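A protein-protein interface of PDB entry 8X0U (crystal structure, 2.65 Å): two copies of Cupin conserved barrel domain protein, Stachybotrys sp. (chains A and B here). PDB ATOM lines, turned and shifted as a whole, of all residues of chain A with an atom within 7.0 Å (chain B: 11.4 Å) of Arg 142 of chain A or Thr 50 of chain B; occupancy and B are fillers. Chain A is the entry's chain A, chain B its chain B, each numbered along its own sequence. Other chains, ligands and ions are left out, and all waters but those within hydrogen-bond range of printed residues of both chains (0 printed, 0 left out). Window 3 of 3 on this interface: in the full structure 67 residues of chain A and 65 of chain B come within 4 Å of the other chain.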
ATOM      1  N   PHE A 132      -3.659 -23.358 -31.825  1.00  0.00           N
ATOM      2  CA  PHE A 132      -3.056 -22.454 -32.789  1.00  0.00           C
ATOM      3  C   PHE A 132      -1.760 -21.882 -32.230  1.00  0.00           C
ATOM      4  O   PHE A 132      -1.588 -21.756 -31.013  1.00  0.00           O
ATOM      5  CB  PHE A 132      -4.012 -21.314 -33.155  1.00  0.00           C
ATOM      6  CG  PHE A 132      -5.111 -21.727 -34.087  1.00  0.00           C
ATOM      7  CD1 PHE A 132      -6.225 -22.397 -33.610  1.00  0.00           C
ATOM      8  CD2 PHE A 132      -5.027 -21.452 -35.442  1.00  0.00           C
ATOM      9  CE1 PHE A 132      -7.236 -22.783 -34.466  1.00  0.00           C
ATOM     10  CE2 PHE A 132      -6.034 -21.833 -36.303  1.00  0.00           C
ATOM     11  CZ  PHE A 132      -7.141 -22.499 -35.816  1.00  0.00           C
ATOM     12  N   LYS A 133      -0.850 -21.539 -33.136  1.00  0.00           N
ATOM     13  CA  LYS A 133       0.414 -20.902 -32.796  1.00  0.00           C
ATOM     14  C   LYS A 133       0.420 -19.498 -33.385  1.00  0.00           C
ATOM     15  O   LYS A 133       0.238 -19.328 -34.596  1.00  0.00           O
ATOM     16  CB  LYS A 133       1.598 -21.716 -33.316  1.00  0.00           C
ATOM     17  CG  LYS A 133       2.955 -21.147 -32.931  1.00  0.00           C
ATOM     18  CD  LYS A 133       4.092 -21.968 -33.513  1.00  0.00           C
ATOM     19  CE  LYS A 133       4.293 -23.264 -32.743  1.00  0.00           C
ATOM     20  NZ  LYS A 133       5.718 -23.706 -32.746  1.00  0.00           N
ATOM     21  N   LEU A 134       0.613 -18.499 -32.527  1.00  0.00           N
ATOM     22  CA  LEU A 134       0.696 -17.103 -32.944  1.00  0.00           C
ATOM     23  C   LEU A 134       2.166 -16.709 -32.993  1.00  0.00           C
ATOM     24  O   LEU A 134       2.838 -16.660 -31.959  1.00  0.00           O
ATOM     25  CB  LEU A 134      -0.090 -16.205 -31.990  1.00  0.00           C
ATOM     26  CG  LEU A 134       0.010 -14.696 -32.215  1.00  0.00           C
ATOM     27  CD1 LEU A 134      -0.628 -14.311 -33.538  1.00  0.00           C
ATOM     28  CD2 LEU A 134      -0.639 -13.939 -31.067  1.00  0.00           C
ATOM     29  N   VAL A 135       2.665 -16.433 -34.196  1.00  0.00           N
ATOM     30  CA  VAL A 135       4.054 -16.053 -34.418  1.00  0.00           C
ATOM     31  C   VAL A 135       4.086 -14.594 -34.844  1.00  0.00           C
ATOM     32  O   VAL A 135       3.307 -14.176 -35.709  1.00  0.00           O
ATOM     33  CB  VAL A 135       4.721 -16.950 -35.477  1.00  0.00           C
ATOM     34  CG1 VAL A 135       6.205 -16.643 -35.572  1.00  0.00           C
ATOM     35  CG2 VAL A 135       4.488 -18.415 -35.152  1.00  0.00           C
ATOM     36  N   LEU A 136       4.982 -13.823 -34.238  1.00  0.00           N
ATOM     37  CA  LEU A 136       5.128 -12.407 -34.538  1.00  0.00           C
ATOM     38  C   LEU A 136       6.343 -12.190 -35.436  1.00  0.00           C
ATOM     39  O   LEU A 136       7.166 -13.084 -35.639  1.00  0.00           O
ATOM     40  CB  LEU A 136       5.244 -11.600 -33.241  1.00  0.00           C
ATOM     41  CG  LEU A 136       4.141 -11.843 -32.205  1.00  0.00           C
ATOM     42  CD1 LEU A 136       4.124 -10.746 -31.157  1.00  0.00           C
ATOM     43  CD2 LEU A 136       2.771 -11.966 -32.859  1.00  0.00           C
ATOM     44  N   GLY A 139       9.782 -13.252 -34.373  1.00  0.00           N
ATOM     45  CA  GLY A 139      10.028 -14.648 -34.098  1.00  0.00           C
ATOM     46  C   GLY A 139       9.486 -15.134 -32.772  1.00  0.00           C
ATOM     47  O   GLY A 139       9.450 -16.351 -32.547  1.00  0.00           O
ATOM     48  N   GLU A 140       9.076 -14.226 -31.888  1.00  0.00           N
ATOM     49  CA  GLU A 140       8.406 -14.633 -30.662  1.00  0.00           C
ATOM     50  C   GLU A 140       7.138 -15.408 -30.998  1.00  0.00           C
ATOM     51  O   GLU A 140       6.500 -15.182 -32.028  1.00  0.00           O
ATOM     52  CB  GLU A 140       8.070 -13.410 -29.807  1.00  0.00           C
ATOM     53  CG  GLU A 140       9.263 -12.517 -29.507  1.00  0.00           C
ATOM     54  CD  GLU A 140       9.008 -11.561 -28.354  1.00  0.00           C
ATOM     55  OE1 GLU A 140       9.987 -10.987 -27.832  1.00  0.00           O
ATOM     56  OE2 GLU A 140       7.833 -11.381 -27.969  1.00  0.00           O
ATOM     57  N   GLU A 141       6.775 -16.339 -30.120  1.00  0.00           N
ATOM     58  CA  GLU A 141       5.654 -17.213 -30.417  1.00  0.00           C
ATOM     59  C   GLU A 141       4.992 -17.676 -29.129  1.00  0.00           C
ATOM     60  O   GLU A 141       5.638 -17.813 -28.086  1.00  0.00           O
ATOM     61  CB  GLU A 141       6.095 -18.420 -31.255  1.00  0.00           C
ATOM     62  CG  GLU A 141       6.781 -19.525 -30.469  1.00  0.00           C
ATOM     63  CD  GLU A 141       7.159 -20.710 -31.340  1.00  0.00           C
ATOM     64  OE1 GLU A 141       7.319 -20.520 -32.566  1.00  0.00           O
ATOM     65  OE2 GLU A 141       7.296 -21.829 -30.797  1.00  0.00           O
ATOM     66  N   ARG A 142       3.685 -17.903 -29.220  1.00  0.00           N
ATOM     67  CA  ARG A 142       2.884 -18.448 -28.138  1.00  0.00           C
ATOM     68  C   ARG A 142       1.974 -19.530 -28.697  1.00  0.00           C
ATOM     69  O   ARG A 142       1.358 -19.352 -29.753  1.00  0.00           O
ATOM     70  CB  ARG A 142       2.034 -17.368 -27.458  1.00  0.00           C
ATOM     71  CG  ARG A 142       2.823 -16.339 -26.679  1.00  0.00           C
ATOM     72  CD  ARG A 142       3.366 -16.916 -25.387  1.00  0.00           C
ATOM     73  NE  ARG A 142       4.024 -15.892 -24.584  1.00  0.00           N
ATOM     74  CZ  ARG A 142       5.223 -15.387 -24.852  1.00  0.00           C
ATOM     75  NH1 ARG A 142       5.903 -15.812 -25.911  1.00  0.00           N
ATOM     76  NH2 ARG A 142       5.742 -14.454 -24.063  1.00  0.00           N
ATOM     77  N   ILE A 143       1.903 -20.651 -27.994  1.00  0.00           N
ATOM     78  CA  ILE A 143       0.942 -21.697 -28.310  1.00  0.00           C
ATOM     79  C   ILE A 143      -0.366 -21.356 -27.613  1.00  0.00           C
ATOM     80  O   ILE A 143      -0.390 -21.107 -26.401  1.00  0.00           O
ATOM     81  CB  ILE A 143       1.461 -23.077 -27.877  1.00  0.00           C
ATOM     82  CG1 ILE A 143       2.653 -23.490 -28.743  1.00  0.00           C
ATOM     83  CG2 ILE A 143       0.351 -24.115 -27.970  1.00  0.00           C
ATOM     84  CD1 ILE A 143       3.468 -24.626 -28.159  1.00  0.00           C
ATOM     85  N   MET A 144      -1.453 -21.322 -28.377  1.00  0.00           N
ATOM     86  CA  MET A 144      -2.760 -20.950 -27.851  1.00  0.00           C
ATOM     87  C   MET A 144      -3.715 -22.122 -28.014  1.00  0.00           C
ATOM     88  O   MET A 144      -3.987 -22.557 -29.139  1.00  0.00           O
ATOM     89  CB  MET A 144      -3.290 -19.695 -28.548  1.00  0.00           C
ATOM     90  CG  MET A 144      -2.473 -18.450 -28.226  1.00  0.00           C
ATOM     91  SD  MET A 144      -3.286 -16.900 -28.645  1.00  0.00           S
ATOM     92  CE  MET A 144      -4.999 -17.316 -28.325  1.00  0.00           C
ATOM     93  N   TRP A 159      -0.928 -16.688 -38.007  1.00  0.00           N
ATOM     94  CA  TRP A 159      -1.553 -17.768 -37.257  1.00  0.00           C
ATOM     95  C   TRP A 159      -1.255 -19.098 -37.933  1.00  0.00           C
ATOM     96  O   TRP A 159      -1.382 -19.222 -39.155  1.00  0.00           O
ATOM     97  CB  TRP A 159      -3.067 -17.561 -37.154  1.00  0.00           C
ATOM     98  CG  TRP A 159      -3.468 -16.358 -36.359  1.00  0.00           C
ATOM     99  CD1 TRP A 159      -3.728 -15.106 -36.838  1.00  0.00           C
ATOM    100  CD2 TRP A 159      -3.660 -16.292 -34.941  1.00  0.00           C
ATOM    101  NE1 TRP A 159      -4.066 -14.265 -35.806  1.00  0.00           N
ATOM    102  CE2 TRP A 159      -4.031 -14.969 -34.631  1.00  0.00           C
ATOM    103  CE3 TRP A 159      -3.555 -17.224 -33.904  1.00  0.00           C
ATOM    104  CZ2 TRP A 159      -4.298 -14.554 -33.328  1.00  0.00           C
ATOM    105  CZ3 TRP A 159      -3.819 -16.809 -32.611  1.00  0.00           C
ATOM    106  CH2 TRP A 159      -4.186 -15.487 -32.335  1.00  0.00           C
ATOM    107  N   GLN B  31      -7.705 -22.629 -15.997  1.00  0.00           N
ATOM    108  CA  GLN B  31      -6.994 -21.360 -15.975  1.00  0.00           C
ATOM    109  C   GLN B  31      -6.619 -20.967 -17.400  1.00  0.00           C
ATOM    110  O   GLN B  31      -6.322 -21.820 -18.242  1.00  0.00           O
ATOM    111  CB  GLN B  31      -5.743 -21.470 -15.100  1.00  0.00           C
ATOM    112  CG  GLN B  31      -4.843 -20.243 -15.101  1.00  0.00           C
ATOM    113  CD  GLN B  31      -5.529 -19.014 -14.540  1.00  0.00           C
ATOM    114  OE1 GLN B  31      -6.131 -18.234 -15.279  1.00  0.00           O
ATOM    115  NE2 GLN B  31      -5.445 -18.835 -13.226  1.00  0.00           N
ATOM    116  N   ILE B  32      -6.641 -19.665 -17.673  1.00  0.00           N
ATOM    117  CA  ILE B  32      -6.471 -19.164 -19.030  1.00  0.00           C
ATOM    118  C   ILE B  32      -5.143 -18.434 -19.160  1.00  0.00           C
ATOM    119  O   ILE B  32      -4.505 -18.043 -18.178  1.00  0.00           O
ATOM    120  CB  ILE B  32      -7.629 -18.238 -19.451  1.00  0.00           C
ATOM    121  CG1 ILE B  32      -7.560 -16.924 -18.672  1.00  0.00           C
ATOM    122  CG2 ILE B  32      -8.966 -18.923 -19.239  1.00  0.00           C
ATOM    123  CD1 ILE B  32      -8.224 -15.773 -19.380  1.00  0.00           C
ATOM    124  N   ASN B  33      -4.726 -18.252 -20.411  1.00  0.00           N
ATOM    125  CA  ASN B  33      -3.598 -17.404 -20.774  1.00  0.00           C
ATOM    126  C   ASN B  33      -4.122 -16.262 -21.631  1.00  0.00           C
ATOM    127  O   ASN B  33      -4.676 -16.498 -22.709  1.00  0.00           O
ATOM    128  CB  ASN B  33      -2.528 -18.191 -21.535  1.00  0.00           C
ATOM    129  CG  ASN B  33      -1.615 -18.972 -20.618  1.00  0.00           C
ATOM    130  OD1 ASN B  33      -1.578 -18.732 -19.413  1.00  0.00           O
ATOM    131  ND2 ASN B  33      -0.861 -19.905 -21.187  1.00  0.00           N
ATOM    132  N   ARG B  34      -3.962 -15.034 -21.150  1.00  0.00           N
ATOM    133  CA  ARG B  34      -4.232 -13.848 -21.949  1.00  0.00           C
ATOM    134  C   ARG B  34      -2.911 -13.336 -22.508  1.00  0.00           C
ATOM    135  O   ARG B  34      -1.987 -13.035 -21.745  1.00  0.00           O
ATOM    136  CB  ARG B  34      -4.921 -12.760 -21.126  1.00  0.00           C
ATOM    137  CG  ARG B  34      -5.047 -11.437 -21.864  1.00  0.00           C
ATOM    138  CD  ARG B  34      -5.636 -10.351 -20.984  1.00  0.00           C
ATOM    139  NE  ARG B  34      -4.704  -9.904 -19.956  1.00  0.00           N
ATOM    140  CZ  ARG B  34      -4.759  -8.712 -19.369  1.00  0.00           C
ATOM    141  NH1 ARG B  34      -5.699  -7.844 -19.710  1.00  0.00           N
ATOM    142  NH2 ARG B  34      -3.867  -8.387 -18.441  1.00  0.00           N
ATOM    143  N   HIS B  35      -2.823 -13.245 -23.831  1.00  0.00           N
ATOM    144  CA  HIS B  35      -1.628 -12.766 -24.513  1.00  0.00           C
ATOM    145  C   HIS B  35      -1.897 -11.384 -25.092  1.00  0.00           C
ATOM    146  O   HIS B  35      -2.859 -11.200 -25.843  1.00  0.00           O
ATOM    147  CB  HIS B  35      -1.199 -13.726 -25.626  1.00  0.00           C
ATOM    148  CG  HIS B  35      -1.018 -15.142 -25.175  1.00  0.00           C
ATOM    149  ND1 HIS B  35       0.034 -15.540 -24.379  1.00  0.00           N
ATOM    150  CD2 HIS B  35      -1.746 -16.257 -25.420  1.00  0.00           C
ATOM    151  CE1 HIS B  35      -0.057 -16.838 -24.147  1.00  0.00           C
ATOM    152  NE2 HIS B  35      -1.130 -17.298 -24.768  1.00  0.00           N
ATOM    153  N   ILE B  36      -1.052 -10.419 -24.738  1.00  0.00           N
ATOM    154  CA  ILE B  36      -1.125  -9.062 -25.265  1.00  0.00           C
ATOM    155  C   ILE B  36       0.131  -8.803 -26.080  1.00  0.00           C
ATOM    156  O   ILE B  36       1.250  -8.981 -25.582  1.00  0.00           O
ATOM    157  CB  ILE B  36      -1.274  -8.023 -24.140  1.00  0.00           C
ATOM    158  CG1 ILE B  36      -2.462  -8.369 -23.243  1.00  0.00           C
ATOM    159  CG2 ILE B  36      -1.437  -6.631 -24.723  1.00  0.00           C
ATOM    160  CD1 ILE B  36      -2.793  -7.294 -22.232  1.00  0.00           C
ATOM    161  N   THR B  37      -0.052  -8.392 -27.332  1.00  0.00           N
ATOM    162  CA  THR B  37       1.059  -8.085 -28.219  1.00  0.00           C
ATOM    163  C   THR B  37       1.280  -6.580 -28.298  1.00  0.00           C
ATOM    164  O   THR B  37       0.423  -5.777 -27.918  1.00  0.00           O
ATOM    165  CB  THR B  37       0.817  -8.648 -29.623  1.00  0.00           C
ATOM    166  OG1 THR B  37      -0.166  -7.852 -30.296  1.00  0.00           O
ATOM    167  CG2 THR B  37       0.338 -10.088 -29.548  1.00  0.00           C
ATOM    168  N   GLY B  38       2.452  -6.210 -28.795  1.00  0.00           N
ATOM    169  CA  GLY B  38       2.798  -4.814 -28.933  1.00  0.00           C
ATOM    170  C   GLY B  38       4.095  -4.660 -29.691  1.00  0.00           C
ATOM    171  O   GLY B  38       4.606  -5.609 -30.288  1.00  0.00           O
ATOM    172  N   SER B  45       7.188  -6.550 -33.578  1.00  0.00           N
ATOM    173  CA  SER B  45       6.019  -7.033 -32.855  1.00  0.00           C
ATOM    174  C   SER B  45       6.450  -8.079 -31.832  1.00  0.00           C
ATOM    175  O   SER B  45       7.044  -9.102 -32.192  1.00  0.00           O
ATOM    176  CB  SER B  45       4.997  -7.613 -33.828  1.00  0.00           C
ATOM    177  OG  SER B  45       4.412  -6.589 -34.612  1.00  0.00           O
ATOM    178  N   VAL B  46       6.147  -7.826 -30.559  1.00  0.00           N
ATOM    179  CA  VAL B  46       6.579  -8.674 -29.455  1.00  0.00           C
ATOM    180  C   VAL B  46       5.407  -8.883 -28.506  1.00  0.00           C
ATOM    181  O   VAL B  46       4.400  -8.173 -28.552  1.00  0.00           O
ATOM    182  CB  VAL B  46       7.782  -8.077 -28.695  1.00  0.00           C
ATOM    183  CG1 VAL B  46       9.008  -8.022 -29.593  1.00  0.00           C
ATOM    184  CG2 VAL B  46       7.437  -6.689 -28.169  1.00  0.00           C
ATOM    185  N   PHE B  47       5.553  -9.877 -27.632  1.00  0.00           N
ATOM    186  CA  PHE B  47       4.546 -10.179 -26.621  1.00  0.00           C
ATOM    187  C   PHE B  47       4.845  -9.361 -25.373  1.00  0.00           C
ATOM    188  O   PHE B  47       5.926  -9.482 -24.788  1.00  0.00           O
ATOM    189  CB  PHE B  47       4.525 -11.671 -26.297  1.00  0.00           C
ATOM    190  CG  PHE B  47       3.893 -12.509 -27.368  1.00  0.00           C
ATOM    191  CD1 PHE B  47       2.518 -12.670 -27.417  1.00  0.00           C
ATOM    192  CD2 PHE B  47       4.670 -13.133 -28.328  1.00  0.00           C
ATOM    193  CE1 PHE B  47       1.929 -13.433 -28.404  1.00  0.00           C
ATOM    194  CE2 PHE B  47       4.086 -13.900 -29.318  1.00  0.00           C
ATOM    195  CZ  PHE B  47       2.712 -14.050 -29.356  1.00  0.00           C
ATOM    196  N   LEU B  48       3.885  -8.529 -24.970  1.00  0.00           N
ATOM    197  CA  LEU B  48       4.095  -7.655 -23.823  1.00  0.00           C
ATOM    198  C   LEU B  48       3.798  -8.365 -22.510  1.00  0.00           C
ATOM    199  O   LEU B  48       4.504  -8.155 -21.518  1.00  0.00           O
ATOM    200  CB  LEU B  48       3.232  -6.401 -23.963  1.00  0.00           C
ATOM    201  CG  LEU B  48       3.596  -5.528 -25.161  1.00  0.00           C
ATOM    202  CD1 LEU B  48       2.543  -4.466 -25.397  1.00  0.00           C
ATOM    203  CD2 LEU B  48       4.959  -4.894 -24.949  1.00  0.00           C
ATOM    204  N   SER B  49       2.769  -9.205 -22.479  1.00  0.00           N
ATOM    205  CA  SER B  49       2.388  -9.845 -21.231  1.00  0.00           C
ATOM    206  C   SER B  49       1.705 -11.176 -21.503  1.00  0.00           C
ATOM    207  O   SER B  49       1.086 -11.379 -22.550  1.00  0.00           O
ATOM    208  CB  SER B  49       1.463  -8.947 -20.404  1.00  0.00           C
ATOM    209  OG  SER B  49       0.338  -8.535 -21.163  1.00  0.00           O
ATOM    210  N   THR B  50       1.837 -12.078 -20.535  1.00  0.00           N
ATOM    211  CA  THR B  50       1.121 -13.348 -20.510  1.00  0.00           C
ATOM    212  C   THR B  50       0.591 -13.511 -19.091  1.00  0.00           C
ATOM    213  O   THR B  50       1.370 -13.736 -18.161  1.00  0.00           O
ATOM    214  CB  THR B  50       2.025 -14.519 -20.890  1.00  0.00           C
ATOM    215  OG1 THR B  50       2.501 -14.342 -22.228  1.00  0.00           O
ATOM    216  CG2 THR B  50       1.254 -15.828 -20.782  1.00  0.00           C
ATOM    217  N   ASP B  51      -0.717 -13.371 -18.913  1.00  0.00           N
ATOM    218  CA  ASP B  51      -1.282 -13.393 -17.573  1.00  0.00           C
ATOM    219  C   ASP B  51      -2.672 -14.021 -17.622  1.00  0.00           C
ATOM    220  O   ASP B  51      -3.090 -14.583 -18.640  1.00  0.00           O
ATOM    221  CB  ASP B  51      -1.307 -11.979 -16.973  1.00  0.00           C
ATOM    222  CG  ASP B  51      -1.934 -10.947 -17.903  1.00  0.00           C
ATOM    223  OD1 ASP B  51      -2.827 -11.298 -18.698  1.00  0.00           O
ATOM    224  OD2 ASP B  51      -1.526  -9.765 -17.824  1.00  0.00           O
ATOM    225  N   HIS B  52      -3.383 -13.917 -16.498  1.00  0.00           N
ATOM    226  CA  HIS B  52      -4.695 -14.519 -16.296  1.00  0.00           C
ATOM    227  C   HIS B  52      -5.824 -13.502 -16.422  1.00  0.00           C
ATOM    228  O   HIS B  52      -6.902 -13.692 -15.852  1.00  0.00           O
ATOM    229  CB  HIS B  52      -4.747 -15.202 -14.927  1.00  0.00           C
ATOM    230  CG  HIS B  52      -4.566 -14.267 -13.766  1.00  0.00           C
ATOM    231  ND1 HIS B  52      -3.827 -13.107 -13.845  1.00  0.00           N
ATOM    232  CD2 HIS B  52      -5.025 -14.329 -12.494  1.00  0.00           C
ATOM    233  CE1 HIS B  52      -3.845 -12.492 -12.676  1.00  0.00           C
ATOM    234  NE2 HIS B  52      -4.566 -13.213 -11.838  1.00  0.00           N
ATOM    235  N   GLY B  53      -5.594 -12.418 -17.156  1.00  0.00           N
ATOM    236  CA  GLY B  53      -6.595 -11.381 -17.283  1.00  0.00           C
ATOM    237  C   GLY B  53      -6.411 -10.267 -16.275  1.00  0.00           C
ATOM    238  O   GLY B  53      -5.289  -9.995 -15.839  1.00  0.00           O
ATOM    239  N   ASP B  54      -7.507  -9.621 -15.887  1.00  0.00           N
ATOM    240  CA  ASP B  54      -7.433  -8.475 -14.995  1.00  0.00           C
ATOM    241  C   ASP B  54      -8.791  -8.263 -14.342  1.00  0.00           C
ATOM    242  O   ASP B  54      -9.824  -8.706 -14.854  1.00  0.00           O
ATOM    243  CB  ASP B  54      -6.993  -7.215 -15.751  1.00  0.00           C
ATOM    244  CG  ASP B  54      -6.205  -6.255 -14.886  1.00  0.00           C
ATOM    245  OD1 ASP B  54      -6.274  -6.381 -13.643  1.00  0.00           O
ATOM    246  OD2 ASP B  54      -5.518  -5.374 -15.452  1.00  0.00           O
ATOM    247  N   HIS B  56     -10.395  -9.335 -11.574  1.00  0.00           N
ATOM    248  CA  HIS B  56     -11.244 -10.426 -11.117  1.00  0.00           C
ATOM    249  C   HIS B  56     -12.236  -9.903 -10.087  1.00  0.00           C
ATOM    250  O   HIS B  56     -11.866  -9.157  -9.176  1.00  0.00           O
ATOM    251  CB  HIS B  56     -10.398 -11.553 -10.524  1.00  0.00           C
ATOM    252  CG  HIS B  56      -9.474 -12.201 -11.507  1.00  0.00           C
ATOM    253  ND1 HIS B  56      -9.455 -11.870 -12.845  1.00  0.00           N
ATOM    254  CD2 HIS B  56      -8.535 -13.165 -11.347  1.00  0.00           C
ATOM    255  CE1 HIS B  56      -8.545 -12.600 -13.466  1.00  0.00           C
ATOM    256  NE2 HIS B  56      -7.972 -13.394 -12.579  1.00  0.00           N
ATOM    257  N   ASN B  67     -13.860 -11.891 -15.158  1.00  0.00           N
ATOM    258  CA  ASN B  67     -12.464 -11.678 -15.533  1.00  0.00           C
ATOM    259  C   ASN B  67     -12.434 -10.737 -16.731  1.00  0.00           C
ATOM    260  O   ASN B  67     -12.778 -11.140 -17.846  1.00  0.00           O
ATOM    261  CB  ASN B  67     -11.780 -13.008 -15.858  1.00  0.00           C
ATOM    262  CG  ASN B  67     -10.316 -12.850 -16.224  1.00  0.00           C
ATOM    263  OD1 ASN B  67      -9.757 -11.755 -16.161  1.00  0.00           O
ATOM    264  ND2 ASN B  67      -9.685 -13.953 -16.608  1.00  0.00           N
ATOM    265  N   LEU B  69     -10.868  -9.234 -19.568  1.00  0.00           N
ATOM    266  CA  LEU B  69      -9.706  -9.560 -20.386  1.00  0.00           C
ATOM    267  C   LEU B  69      -9.126  -8.328 -21.068  1.00  0.00           C
ATOM    268  O   LEU B  69      -7.903  -8.212 -21.204  1.00  0.00           O
ATOM    269  CB  LEU B  69     -10.082 -10.623 -21.415  1.00  0.00           C
ATOM    270  CG  LEU B  69     -10.582 -11.913 -20.765  1.00  0.00           C
ATOM    271  CD1 LEU B  69     -10.933 -12.957 -21.806  1.00  0.00           C
ATOM    272  CD2 LEU B  69      -9.539 -12.443 -19.795  1.00  0.00           C
ATOM    273  N   TYR B  70      -9.974  -7.400 -21.504  1.00  0.00           N
ATOM    274  CA  TYR B  70      -9.487  -6.141 -22.047  1.00  0.00           C
ATOM    275  C   TYR B  70     -10.625  -5.133 -22.071  1.00  0.00           C
ATOM    276  O   TYR B  70     -11.785  -5.465 -21.818  1.00  0.00           O
ATOM    277  CB  TYR B  70      -8.896  -6.311 -23.449  1.00  0.00           C
ATOM    278  CG  TYR B  70      -7.737  -5.378 -23.701  1.00  0.00           C
ATOM    279  CD1 TYR B  70      -6.502  -5.604 -23.107  1.00  0.00           C
ATOM    280  CD2 TYR B  70      -7.881  -4.260 -24.512  1.00  0.00           C
ATOM    281  CE1 TYR B  70      -5.439  -4.754 -23.323  1.00  0.00           C
ATOM    282  CE2 TYR B  70      -6.819  -3.402 -24.736  1.00  0.00           C
ATOM    283  CZ  TYR B  70      -5.600  -3.654 -24.137  1.00  0.00           C
ATOM    284  OH  TYR B  70      -4.540  -2.806 -24.355  1.00  0.00           O
ATOM    285  N   ILE B  85      -3.176   0.181 -22.876  1.00  0.00           N
ATOM    286  CA  ILE B  85      -2.857  -0.812 -21.856  1.00  0.00           C
ATOM    287  C   ILE B  85      -3.030  -0.220 -20.463  1.00  0.00           C
ATOM    288  O   ILE B  85      -3.652  -0.829 -19.584  1.00  0.00           O
ATOM    289  CB  ILE B  85      -1.432  -1.353 -22.063  1.00  0.00           C
ATOM    290  CG1 ILE B  85      -1.349  -2.157 -23.361  1.00  0.00           C
ATOM    291  CG2 ILE B  85      -1.010  -2.203 -20.875  1.00  0.00           C
ATOM    292  CD1 ILE B  85       0.034  -2.672 -23.661  1.00  0.00           C
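The backbone NH (N) of Phe 47 of chain B sits at hydrogen-bond distance from the side-chain carboxylate (OE2) of Glu 140 of chain A, 2.8 Å away.
The guanidinium group of Arg 142 of chain A lies within hydrogen-bond range of the side-chain hydroxyl of Thr 50 of chain B, 3.2 Å away.
O of Phe 132 of chain A sits at hydrogen-bond distance from N of Met 144 of chain A (2.7 Å).
The side-chain amino group of Lys 133 of chain A is in salt-bridge range of the side-chain carboxylate of Glu 141 of chain A (3.1 Å).
O of Arg 142 of chain A lies within hydrogen-bond range of N of Leu 134 of chain A, 3.0 Å away.
The side-chain hydroxyl of Thr 50 of chain B lies within hydrogen-bond range of a ring nitrogen (ND1) of His 35 of chain B, 3.5 Å away.
O of Gly 38 of chain B is in hydrogen-bond range of N of Val 46 of chain B (2.7 Å).
Among the printed residues, merely in contact across the chains: Leu 136 of chain A with Ser 45 of chain B (3.3 Å), Glu 140 of chain A with Val 46 of chain B (3.3 Å), Leu 136 of chain A with Val 46 of chain B (3.5 Å), Arg 142 of chain A with Phe 47 of chain B (3.5 Å), Leu 136 of chain A with Phe 47 of chain B (3.5 Å), Met 144 of chain A with His 35 of chain B (3.6 Å), Arg 142 of chain A with His 35 of chain B (3.6 Å), Leu 134 of chain A with Phe 47 of chain B (3.7 Å) and Glu 141 of chain A with Phe 47 of chain B (3.7 Å).
No residue of chain B comes within 4 Å of Lys 133 of chain A.
Printed residues of chain B within 4 Å of Leu 134 of chain A: Phe 47.
Printed residues of chain B within 4 Å of Leu 136 of chain A: Ser 45, Val 46 and Phe 47.
Of chain B, only Val 46 and Phe 47 come within 4 Å of Glu 140 of chain A.
Glu 141 of chain A touches one residue of chain B.
Of chain B, only His 35, Phe 47 and Thr 50 come within 4 Å of Arg 142 of chain A.
No residue of chain B comes within 4 Å of Ile 143 of chain A.
Of chain B, only His 35 comes within 4 Å of Met 144 of chain A.
Of the printed residues of chain A, His 35 of chain B touches Arg 142 and Met 144.
Of the printed residues of chain A, Ser 45 of chain B touches Leu 136 (3.3 Å).
Of the printed residues of chain A, Val 46 of chain B touches Leu 136 (3.5 Å) and Glu 140 (3.3 Å).
Of the printed residues of chain A, Phe 47 of chain B touches Leu 134 (3.7 Å), Leu 136 (3.5 Å), Glu 140 (2.8 Å), Glu 141 (3.7 Å) and Arg 142 (3.5 Å).
Thr 50 of chain B touches one residue of chain A.
The nearest printed residue of chain A that does not touch Val 46 of chain B is Gly 139 of chain A (7.1 Å).
Of the 12 printed residues of chain A, 6 touch a printed residue of chain B.
Hydrophobic or aromatic side chains of chain A within 4 Å of the printed part of chain B: Leu 134, Leu 136 and Met 144.
Among the printed residues, 11 pairs touch across the chains.
Among the printed residues, no Asp or Glu carboxylate lies within 4 Å of a Lys or Arg side-chain nitrogen of the other chain.
No position is printed for both chains.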
